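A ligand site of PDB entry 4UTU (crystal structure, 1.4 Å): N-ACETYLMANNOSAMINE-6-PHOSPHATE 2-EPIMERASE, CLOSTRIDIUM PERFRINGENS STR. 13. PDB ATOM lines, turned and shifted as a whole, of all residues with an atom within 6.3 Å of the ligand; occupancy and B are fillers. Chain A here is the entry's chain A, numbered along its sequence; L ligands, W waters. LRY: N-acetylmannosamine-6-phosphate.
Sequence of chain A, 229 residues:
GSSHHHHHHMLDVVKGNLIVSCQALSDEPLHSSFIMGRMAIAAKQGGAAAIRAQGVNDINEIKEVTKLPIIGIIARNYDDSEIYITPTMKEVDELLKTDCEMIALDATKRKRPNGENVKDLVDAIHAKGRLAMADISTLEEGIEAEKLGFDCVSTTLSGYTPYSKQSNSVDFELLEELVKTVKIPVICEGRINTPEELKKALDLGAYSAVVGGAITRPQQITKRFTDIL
The side-chain carboxylate (OE2) of Glu 189 is in hydrogen-bond range of an oxygen (O5) of the ligand, 2.6 Å away. O7 of the ligand sits at hydrogen-bond distance from OH of Tyr 84 (2.6 Å). The backbone NH of Arg 191 sits at hydrogen-bond distance from an oxygen (OP1) of the ligand (2.8 Å). N of Gly 212 is in hydrogen-bond range of OP2 of the ligand (2.8 Å). The backbone NH (N) of Gly 213 lies within hydrogen-bond range of an oxygen (OP3) of the ligand (2.9 Å). The side-chain amide nitrogen (NE2) of Gln 23 sits at hydrogen-bond distance from an oxygen (O1) of the ligand. An oxygen (O4) of the ligand is in hydrogen-bond range of the guanidinium group (NH1) of Arg 217, at 3.0 Å. NE of Arg 52 lies within hydrogen-bond range of O1 of the ligand, 3.0 Å away.
Ile 73 touches the ligand. Ile 85 touches the ligand (CD1 to O7, 3.97 Å). CG2 of Thr 156 touches O5 of the ligand, at 3.7 Å. CD2 of Tyr 160 touches C8 of the ligand, 3.5 Å away. Gly 190 touches the ligand. Val 211 touches the ligand. Within 4 Å of the ligand: Gln 23, Arg 52, Ile 73, Tyr 84, Ile 85, Thr 156, Tyr 160, Glu 189, Gly 190, Arg 191, Val 211, Gly 212, Gly 213 and Arg 217. The nearest printed residue that does not touch the ligand is Ser 21 (4.01 Å).
OE1 of Glu 189 is in salt-bridge range of NH1 of Arg 52. OE1 of Glu 189 sits close to OG1 of Thr 156, 3.0 Å away. The side-chain hydroxyl (OG) of Ser 21 lies within hydrogen-bond range of the side-chain amide nitrogen (NE2) of Gln 23 (2.8 Å). NH2 of Arg 52 is in salt-bridge range of OD2 of Asp 135 (2.7 Å). OG1 of Thr 156 sits at hydrogen-bond distance from OD1 of Asp 135 (3.0 Å). O of Val 211 lies within hydrogen-bond range of N of Ser 21, at 2.9 Å.
Water W6 lies within hydrogen-bond range of OP3 of the ligand (2.6 Å), OE1 of Gln 220 (2.8 Å) and NH1 of Arg 217 (3.0 Å). Water W10 lies within hydrogen-bond range of OP1 of the ligand (2.7 Å) and OH of Tyr 160 (2.7 Å). Water W1 bridges OP1 of the ligand (2.7 Å) and NE2 of Gln 220 (3.3 Å). Water W2 bridges the side-chain hydroxyl of Ser 21 (2.6 Å) and an oxygen (O4) of the ligand (2.7 Å). Water W8 bridges an oxygen (O5) of the ligand (2.8 Å) and the backbone carbonyl oxygen of Thr 156 (2.8 Å). Water W9 lies within hydrogen-bond range of OE1 of Gln 23, O3 of the ligand and NH2 of Arg 217.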
ATOM      1  N   SER A  21     -26.489 -30.261  14.118  1.00  0.00           N
ATOM      2  CA  SER A  21     -27.067 -28.978  14.379  1.00  0.00           C
ATOM      3  C   SER A  21     -28.584 -29.024  14.274  1.00  0.00           C
ATOM      4  O   SER A  21     -29.120 -29.442  13.225  1.00  0.00           O
ATOM      5  CB  SER A  21     -26.403 -27.945  13.479  1.00  0.00           C
ATOM      6  OG  SER A  21     -26.947 -26.628  13.683  1.00  0.00           O
ATOM      7  N   GLN A  23     -31.431 -26.599  14.554  1.00  0.00           N
ATOM      8  CA  GLN A  23     -31.838 -25.205  14.553  1.00  0.00           C
ATOM      9  C   GLN A  23     -33.093 -25.000  13.682  1.00  0.00           C
ATOM     10  O   GLN A  23     -33.261 -25.616  12.614  1.00  0.00           O
ATOM     11  CB  GLN A  23     -30.726 -24.255  14.113  1.00  0.00           C
ATOM     12  CG  GLN A  23     -29.509 -24.311  14.984  1.00  0.00           C
ATOM     13  CD  GLN A  23     -28.421 -23.398  14.487  1.00  0.00           C
ATOM     14  OE1 GLN A  23     -28.697 -22.242  14.197  1.00  0.00           O
ATOM     15  NE2 GLN A  23     -27.174 -23.893  14.433  1.00  0.00           N
ATOM     16  N   LEU A  25     -35.070 -21.271  12.887  1.00  0.00           N
ATOM     17  CA  LEU A  25     -35.265 -19.854  13.222  1.00  0.00           C
ATOM     18  C   LEU A  25     -36.715 -19.472  13.025  1.00  0.00           C
ATOM     19  O   LEU A  25     -37.528 -20.279  12.614  1.00  0.00           O
ATOM     20  CB  LEU A  25     -34.265 -18.963  12.446  1.00  0.00           C
ATOM     21  CG  LEU A  25     -32.793 -19.383  12.626  1.00  0.00           C
ATOM     22  CD1 LEU A  25     -31.854 -18.421  11.863  1.00  0.00           C
ATOM     23  CD2 LEU A  25     -32.385 -19.449  14.109  1.00  0.00           C
ATOM     24  N   ARG A  52     -25.333 -28.917  18.077  1.00  0.00           N
ATOM     25  CA  ARG A  52     -25.208 -27.470  17.944  1.00  0.00           C
ATOM     26  C   ARG A  52     -26.601 -26.876  17.905  1.00  0.00           C
ATOM     27  O   ARG A  52     -27.488 -27.429  17.248  1.00  0.00           O
ATOM     28  CB  ARG A  52     -24.427 -27.117  16.661  1.00  0.00           C
ATOM     29  CG  ARG A  52     -24.245 -25.603  16.480  1.00  0.00           C
ATOM     30  CD  ARG A  52     -23.223 -25.290  15.431  1.00  0.00           C
ATOM     31  NE  ARG A  52     -23.238 -23.871  15.083  1.00  0.00           N
ATOM     32  CZ  ARG A  52     -22.168 -23.107  14.881  1.00  0.00           C
ATOM     33  NH1 ARG A  52     -20.946 -23.598  14.922  1.00  0.00           N
ATOM     34  NH2 ARG A  52     -22.371 -21.816  14.586  1.00  0.00           N
ATOM     35  N   ILE A  73     -25.087 -21.186  20.292  1.00  0.00           N
ATOM     36  CA  ILE A  73     -25.008 -19.850  19.688  1.00  0.00           C
ATOM     37  C   ILE A  73     -26.292 -19.092  19.937  1.00  0.00           C
ATOM     38  O   ILE A  73     -27.327 -19.676  20.257  1.00  0.00           O
ATOM     39  CB  ILE A  73     -24.750 -19.918  18.162  1.00  0.00           C
ATOM     40  CG1 ILE A  73     -25.966 -20.461  17.373  1.00  0.00           C
ATOM     41  CG2 ILE A  73     -23.413 -20.667  17.866  1.00  0.00           C
ATOM     42  CD1 ILE A  73     -25.936 -20.299  15.861  1.00  0.00           C
ATOM     43  N   TYR A  84     -23.859 -11.938  12.813  1.00  0.00           N
ATOM     44  CA  TYR A  84     -25.072 -12.376  13.517  1.00  0.00           C
ATOM     45  C   TYR A  84     -24.856 -13.586  14.433  1.00  0.00           C
ATOM     46  O   TYR A  84     -25.691 -13.833  15.276  1.00  0.00           O
ATOM     47  CB  TYR A  84     -26.239 -12.651  12.537  1.00  0.00           C
ATOM     48  CG  TYR A  84     -25.973 -13.745  11.576  1.00  0.00           C
ATOM     49  CD1 TYR A  84     -25.356 -13.487  10.356  1.00  0.00           C
ATOM     50  CD2 TYR A  84     -26.292 -15.044  11.899  1.00  0.00           C
ATOM     51  CE1 TYR A  84     -25.120 -14.525   9.462  1.00  0.00           C
ATOM     52  CE2 TYR A  84     -26.013 -16.076  11.024  1.00  0.00           C
ATOM     53  CZ  TYR A  84     -25.413 -15.802   9.814  1.00  0.00           C
ATOM     54  OH  TYR A  84     -25.102 -16.847   8.934  1.00  0.00           O
ATOM     55  N   ILE A  85     -23.761 -14.338  14.286  1.00  0.00           N
ATOM     56  CA  ILE A  85     -23.540 -15.506  15.157  1.00  0.00           C
ATOM     57  C   ILE A  85     -22.808 -15.044  16.407  1.00  0.00           C
ATOM     58  O   ILE A  85     -21.598 -14.749  16.332  1.00  0.00           O
ATOM     59  CB  ILE A  85     -22.741 -16.668  14.456  1.00  0.00           C
ATOM     60  CG1 ILE A  85     -23.474 -17.116  13.203  1.00  0.00           C
ATOM     61  CG2 ILE A  85     -22.555 -17.837  15.442  1.00  0.00           C
ATOM     62  CD1 ILE A  85     -22.832 -18.298  12.471  1.00  0.00           C
ATOM     63  N   ASP A 135     -16.266 -19.564  14.364  1.00  0.00           N
ATOM     64  CA  ASP A 135     -16.913 -19.755  13.061  1.00  0.00           C
ATOM     65  C   ASP A 135     -16.248 -18.791  12.075  1.00  0.00           C
ATOM     66  O   ASP A 135     -16.334 -17.569  12.231  1.00  0.00           O
ATOM     67  CB  ASP A 135     -18.436 -19.460  13.102  1.00  0.00           C
ATOM     68  CG  ASP A 135     -19.228 -20.490  13.892  1.00  0.00           C
ATOM     69  OD1 ASP A 135     -18.777 -21.651  14.016  1.00  0.00           O
ATOM     70  OD2 ASP A 135     -20.302 -20.111  14.392  1.00  0.00           O
ATOM     71  N   THR A 156     -17.923 -22.946   9.260  1.00  0.00           N
ATOM     72  CA  THR A 156     -19.299 -22.527   9.246  1.00  0.00           C
ATOM     73  C   THR A 156     -19.684 -21.411   8.291  1.00  0.00           C
ATOM     74  O   THR A 156     -20.743 -21.470   7.641  1.00  0.00           O
ATOM     75  CB  THR A 156     -19.682 -22.055  10.670  1.00  0.00           C
ATOM     76  OG1 THR A 156     -19.468 -23.156  11.556  1.00  0.00           O
ATOM     77  CG2 THR A 156     -21.158 -21.624  10.784  1.00  0.00           C
ATOM     78  N   LEU A 157     -18.871 -20.370   8.267  1.00  0.00           N
ATOM     79  CA  LEU A 157     -19.247 -19.139   7.548  1.00  0.00           C
ATOM     80  C   LEU A 157     -18.658 -19.032   6.137  1.00  0.00           C
ATOM     81  O   LEU A 157     -18.888 -18.086   5.421  1.00  0.00           O
ATOM     82  CB  LEU A 157     -18.901 -17.904   8.386  1.00  0.00           C
ATOM     83  CG  LEU A 157     -19.898 -17.669   9.515  1.00  0.00           C
ATOM     84  CD1 LEU A 157     -19.353 -16.602  10.440  1.00  0.00           C
ATOM     85  CD2 LEU A 157     -21.308 -17.257   9.001  1.00  0.00           C
ATOM     86  N   TYR A 160     -20.734 -17.657   3.301  1.00  0.00           N
ATOM     87  CA  TYR A 160     -21.751 -16.837   3.979  1.00  0.00           C
ATOM     88  C   TYR A 160     -21.169 -15.453   4.330  1.00  0.00           C
ATOM     89  O   TYR A 160     -21.752 -14.701   5.133  1.00  0.00           O
ATOM     90  CB  TYR A 160     -22.313 -17.588   5.178  1.00  0.00           C
ATOM     91  CG  TYR A 160     -22.892 -18.903   4.806  1.00  0.00           C
ATOM     92  CD1 TYR A 160     -24.110 -18.965   4.168  1.00  0.00           C
ATOM     93  CD2 TYR A 160     -22.256 -20.080   5.063  1.00  0.00           C
ATOM     94  CE1 TYR A 160     -24.614 -20.158   3.765  1.00  0.00           C
ATOM     95  CE2 TYR A 160     -22.784 -21.257   4.675  1.00  0.00           C
ATOM     96  CZ  TYR A 160     -23.958 -21.325   4.059  1.00  0.00           C
ATOM     97  OH  TYR A 160     -24.485 -22.536   3.614  1.00  0.00           O
ATOM     98  N   GLU A 189     -17.929 -27.618   8.835  1.00  0.00           N
ATOM     99  CA  GLU A 189     -19.323 -27.242   9.038  1.00  0.00           C
ATOM    100  C   GLU A 189     -19.834 -26.368   7.879  1.00  0.00           C
ATOM    101  O   GLU A 189     -19.250 -25.315   7.590  1.00  0.00           O
ATOM    102  CB  GLU A 189     -19.477 -26.493  10.379  1.00  0.00           C
ATOM    103  CG  GLU A 189     -20.916 -26.024  10.661  1.00  0.00           C
ATOM    104  CD  GLU A 189     -21.154 -25.529  12.069  1.00  0.00           C
ATOM    105  OE1 GLU A 189     -20.276 -25.734  12.956  1.00  0.00           O
ATOM    106  OE2 GLU A 189     -22.220 -24.921  12.317  1.00  0.00           O
ATOM    107  N   GLY A 190     -20.861 -26.822   7.199  1.00  0.00           N
ATOM    108  CA  GLY A 190     -21.474 -26.093   6.120  1.00  0.00           C
ATOM    109  C   GLY A 190     -21.679 -26.913   4.856  1.00  0.00           C
ATOM    110  O   GLY A 190     -20.734 -27.291   4.200  1.00  0.00           O
ATOM    111  N   ARG A 191     -22.941 -27.209   4.568  1.00  0.00           N
ATOM    112  CA  ARG A 191     -23.367 -27.785   3.308  1.00  0.00           C
ATOM    113  C   ARG A 191     -22.973 -29.220   3.123  1.00  0.00           C
ATOM    114  O   ARG A 191     -23.020 -29.715   2.032  1.00  0.00           O
ATOM    115  CB  ARG A 191     -23.000 -26.899   2.142  1.00  0.00           C
ATOM    116  CG  ARG A 191     -23.495 -25.453   2.249  1.00  0.00           C
ATOM    117  CD  ARG A 191     -23.192 -24.553   1.067  1.00  0.00           C
ATOM    118  NE  ARG A 191     -21.782 -24.460   0.814  1.00  0.00           N
ATOM    119  CZ  ARG A 191     -20.979 -23.538   1.295  1.00  0.00           C
ATOM    120  NH1 ARG A 191     -21.407 -22.474   1.937  1.00  0.00           N
ATOM    121  NH2 ARG A 191     -19.687 -23.639   1.063  1.00  0.00           N
ATOM    122  N   ILE A 192     -22.668 -29.935   4.221  1.00  0.00           N
ATOM    123  CA  ILE A 192     -22.491 -31.402   4.171  1.00  0.00           C
ATOM    124  C   ILE A 192     -23.847 -32.040   3.917  1.00  0.00           C
ATOM    125  O   ILE A 192     -24.708 -31.993   4.822  1.00  0.00           O
ATOM    126  CB  ILE A 192     -21.846 -31.989   5.430  1.00  0.00           C
ATOM    127  CG1 ILE A 192     -20.468 -31.390   5.668  1.00  0.00           C
ATOM    128  CG2 ILE A 192     -21.823 -33.523   5.264  1.00  0.00           C
ATOM    129  CD1 ILE A 192     -19.839 -31.723   7.039  1.00  0.00           C
ATOM    130  N   VAL A 210     -19.955 -30.983  11.554  1.00  0.00           N
ATOM    131  CA  VAL A 210     -21.303 -30.615  11.910  1.00  0.00           C
ATOM    132  C   VAL A 210     -22.195 -30.706  10.691  1.00  0.00           C
ATOM    133  O   VAL A 210     -21.852 -30.156   9.659  1.00  0.00           O
ATOM    134  CB  VAL A 210     -21.370 -29.163  12.458  1.00  0.00           C
ATOM    135  CG1 VAL A 210     -22.822 -28.738  12.744  1.00  0.00           C
ATOM    136  CG2 VAL A 210     -20.488 -28.994  13.702  1.00  0.00           C
ATOM    137  N   VAL A 211     -23.306 -31.427  10.840  1.00  0.00           N
ATOM    138  CA  VAL A 211     -24.361 -31.516   9.834  1.00  0.00           C
ATOM    139  C   VAL A 211     -25.621 -30.948  10.448  1.00  0.00           C
ATOM    140  O   VAL A 211     -26.057 -31.464  11.475  1.00  0.00           O
ATOM    141  CB  VAL A 211     -24.555 -32.955   9.314  1.00  0.00           C
ATOM    142  CG1 VAL A 211     -25.770 -33.014   8.378  1.00  0.00           C
ATOM    143  CG2 VAL A 211     -23.284 -33.537   8.666  1.00  0.00           C
ATOM    144  N   GLY A 212     -26.212 -29.967   9.763  1.00  0.00           N
ATOM    145  CA  GLY A 212     -27.449 -29.393  10.185  1.00  0.00           C
ATOM    146  C   GLY A 212     -28.597 -29.687   9.278  1.00  0.00           C
ATOM    147  O   GLY A 212     -29.328 -30.692   9.478  1.00  0.00           O
ATOM    148  N   GLY A 213     -28.772 -28.875   8.250  1.00  0.00           N
ATOM    149  CA  GLY A 213     -29.970 -28.955   7.448  1.00  0.00           C
ATOM    150  C   GLY A 213     -30.269 -30.293   6.789  1.00  0.00           C
ATOM    151  O   GLY A 213     -31.422 -30.616   6.605  1.00  0.00           O
ATOM    152  N   ALA A 214     -29.231 -31.018   6.379  1.00  0.00           N
ATOM    153  CA  ALA A 214     -29.392 -32.298   5.739  1.00  0.00           C
ATOM    154  C   ALA A 214     -30.000 -33.325   6.675  1.00  0.00           C
ATOM    155  O   ALA A 214     -30.420 -34.381   6.200  1.00  0.00           O
ATOM    156  CB  ALA A 214     -28.074 -32.810   5.126  1.00  0.00           C
ATOM    157  N   ARG A 217     -33.539 -30.004   8.729  1.00  0.00           N
ATOM    158  CA  ARG A 217     -34.375 -29.079   7.974  1.00  0.00           C
ATOM    159  C   ARG A 217     -35.092 -29.814   6.835  1.00  0.00           C
ATOM    160  O   ARG A 217     -34.630 -29.810   5.675  1.00  0.00           O
ATOM    161  CB  ARG A 217     -33.557 -27.899   7.404  1.00  0.00           C
ATOM    162  CG  ARG A 217     -33.158 -26.897   8.490  1.00  0.00           C
ATOM    163  CD  ARG A 217     -32.327 -25.755   7.939  1.00  0.00           C
ATOM    164  NE  ARG A 217     -32.340 -24.657   8.892  1.00  0.00           N
ATOM    165  CZ  ARG A 217     -31.313 -24.034   9.411  1.00  0.00           C
ATOM    166  NH1 ARG A 217     -30.077 -24.341   9.085  1.00  0.00           N
ATOM    167  NH2 ARG A 217     -31.536 -23.097  10.331  1.00  0.00           N
ATOM    168  N   GLN A 220     -35.409 -28.159   3.425  1.00  0.00           N
ATOM    169  CA  GLN A 220     -34.213 -28.188   2.610  1.00  0.00           C
ATOM    170  C   GLN A 220     -33.967 -29.565   2.002  1.00  0.00           C
ATOM    171  O   GLN A 220     -33.613 -29.687   0.836  1.00  0.00           O
ATOM    172  CB  GLN A 220     -33.044 -27.802   3.501  1.00  0.00           C
ATOM    173  CG  GLN A 220     -31.669 -27.885   2.910  1.00  0.00           C
ATOM    174  CD  GLN A 220     -30.563 -27.672   3.932  1.00  0.00           C
ATOM    175  OE1 GLN A 220     -30.615 -26.714   4.711  1.00  0.00           O
ATOM    176  NE2 GLN A 220     -29.537 -28.496   3.882  1.00  0.00           N
HETATM  177  N   LRY L   1     -24.861 -21.369   9.707  1.00  0.00           N
HETATM  178  P   LRY L   1     -25.513 -26.984   7.508  1.00  0.00           P
HETATM  179  C1  LRY L   1     -24.636 -22.080  11.954  1.00  0.00           C
HETATM  180  O1  LRY L   1     -24.977 -22.525  13.040  1.00  0.00           O
HETATM  181  C2  LRY L   1     -25.599 -21.786  10.876  1.00  0.00           C
HETATM  182  C3  LRY L   1     -26.623 -22.890  10.651  1.00  0.00           C
HETATM  183  O3  LRY L   1     -27.664 -22.314   9.873  1.00  0.00           O
HETATM  184  C4  LRY L   1     -26.121 -24.102   9.894  1.00  0.00           C
HETATM  185  O4  LRY L   1     -27.268 -24.983   9.748  1.00  0.00           O
HETATM  186  C5  LRY L   1     -25.069 -24.906  10.584  1.00  0.00           C
HETATM  187  O5  LRY L   1     -23.859 -24.108  10.454  1.00  0.00           O
HETATM  188  C6  LRY L   1     -24.775 -26.251   9.937  1.00  0.00           C
HETATM  189  O6  LRY L   1     -24.665 -26.129   8.510  1.00  0.00           O
HETATM  190  C7  LRY L   1     -24.948 -20.122   9.260  1.00  0.00           C
HETATM  191  O7  LRY L   1     -25.636 -19.262   9.828  1.00  0.00           O
HETATM  192  C8  LRY L   1     -24.228 -19.816   7.986  1.00  0.00           C
HETATM  193  OP1 LRY L   1     -25.161 -26.403   6.136  1.00  0.00           O
HETATM  194  OP2 LRY L   1     -25.112 -28.411   7.664  1.00  0.00           O
HETATM  195  OP3 LRY L   1     -26.960 -26.706   7.849  1.00  0.00           O
HETATM  196  O   HOH W   1     -26.993 -26.491   4.168  1.00  0.00           O
HETATM  197  O   HOH W   2     -28.694 -26.041  11.823  1.00  0.00           O
HETATM  198  O   HOH W   3     -22.543 -29.167   7.226  1.00  0.00           O
HETATM  199  O   HOH W   4     -28.299 -18.899  11.015  1.00  0.00           O
HETATM  200  O   HOH W   5     -26.883 -22.081   7.024  1.00  0.00           O
HETATM  201  O   HOH W   6     -28.987 -25.533   6.611  1.00  0.00           O
HETATM  202  O   HOH W   7     -26.401 -30.212   5.992  1.00  0.00           O
HETATM  203  O   HOH W   8     -23.025 -23.083   8.009  1.00  0.00           O
HETATM  204  O   HOH W   9     -29.564 -21.379  11.722  1.00  0.00           O
HETATM  205  O   HOH W  10     -24.757 -23.748   6.052  1.00  0.00           O
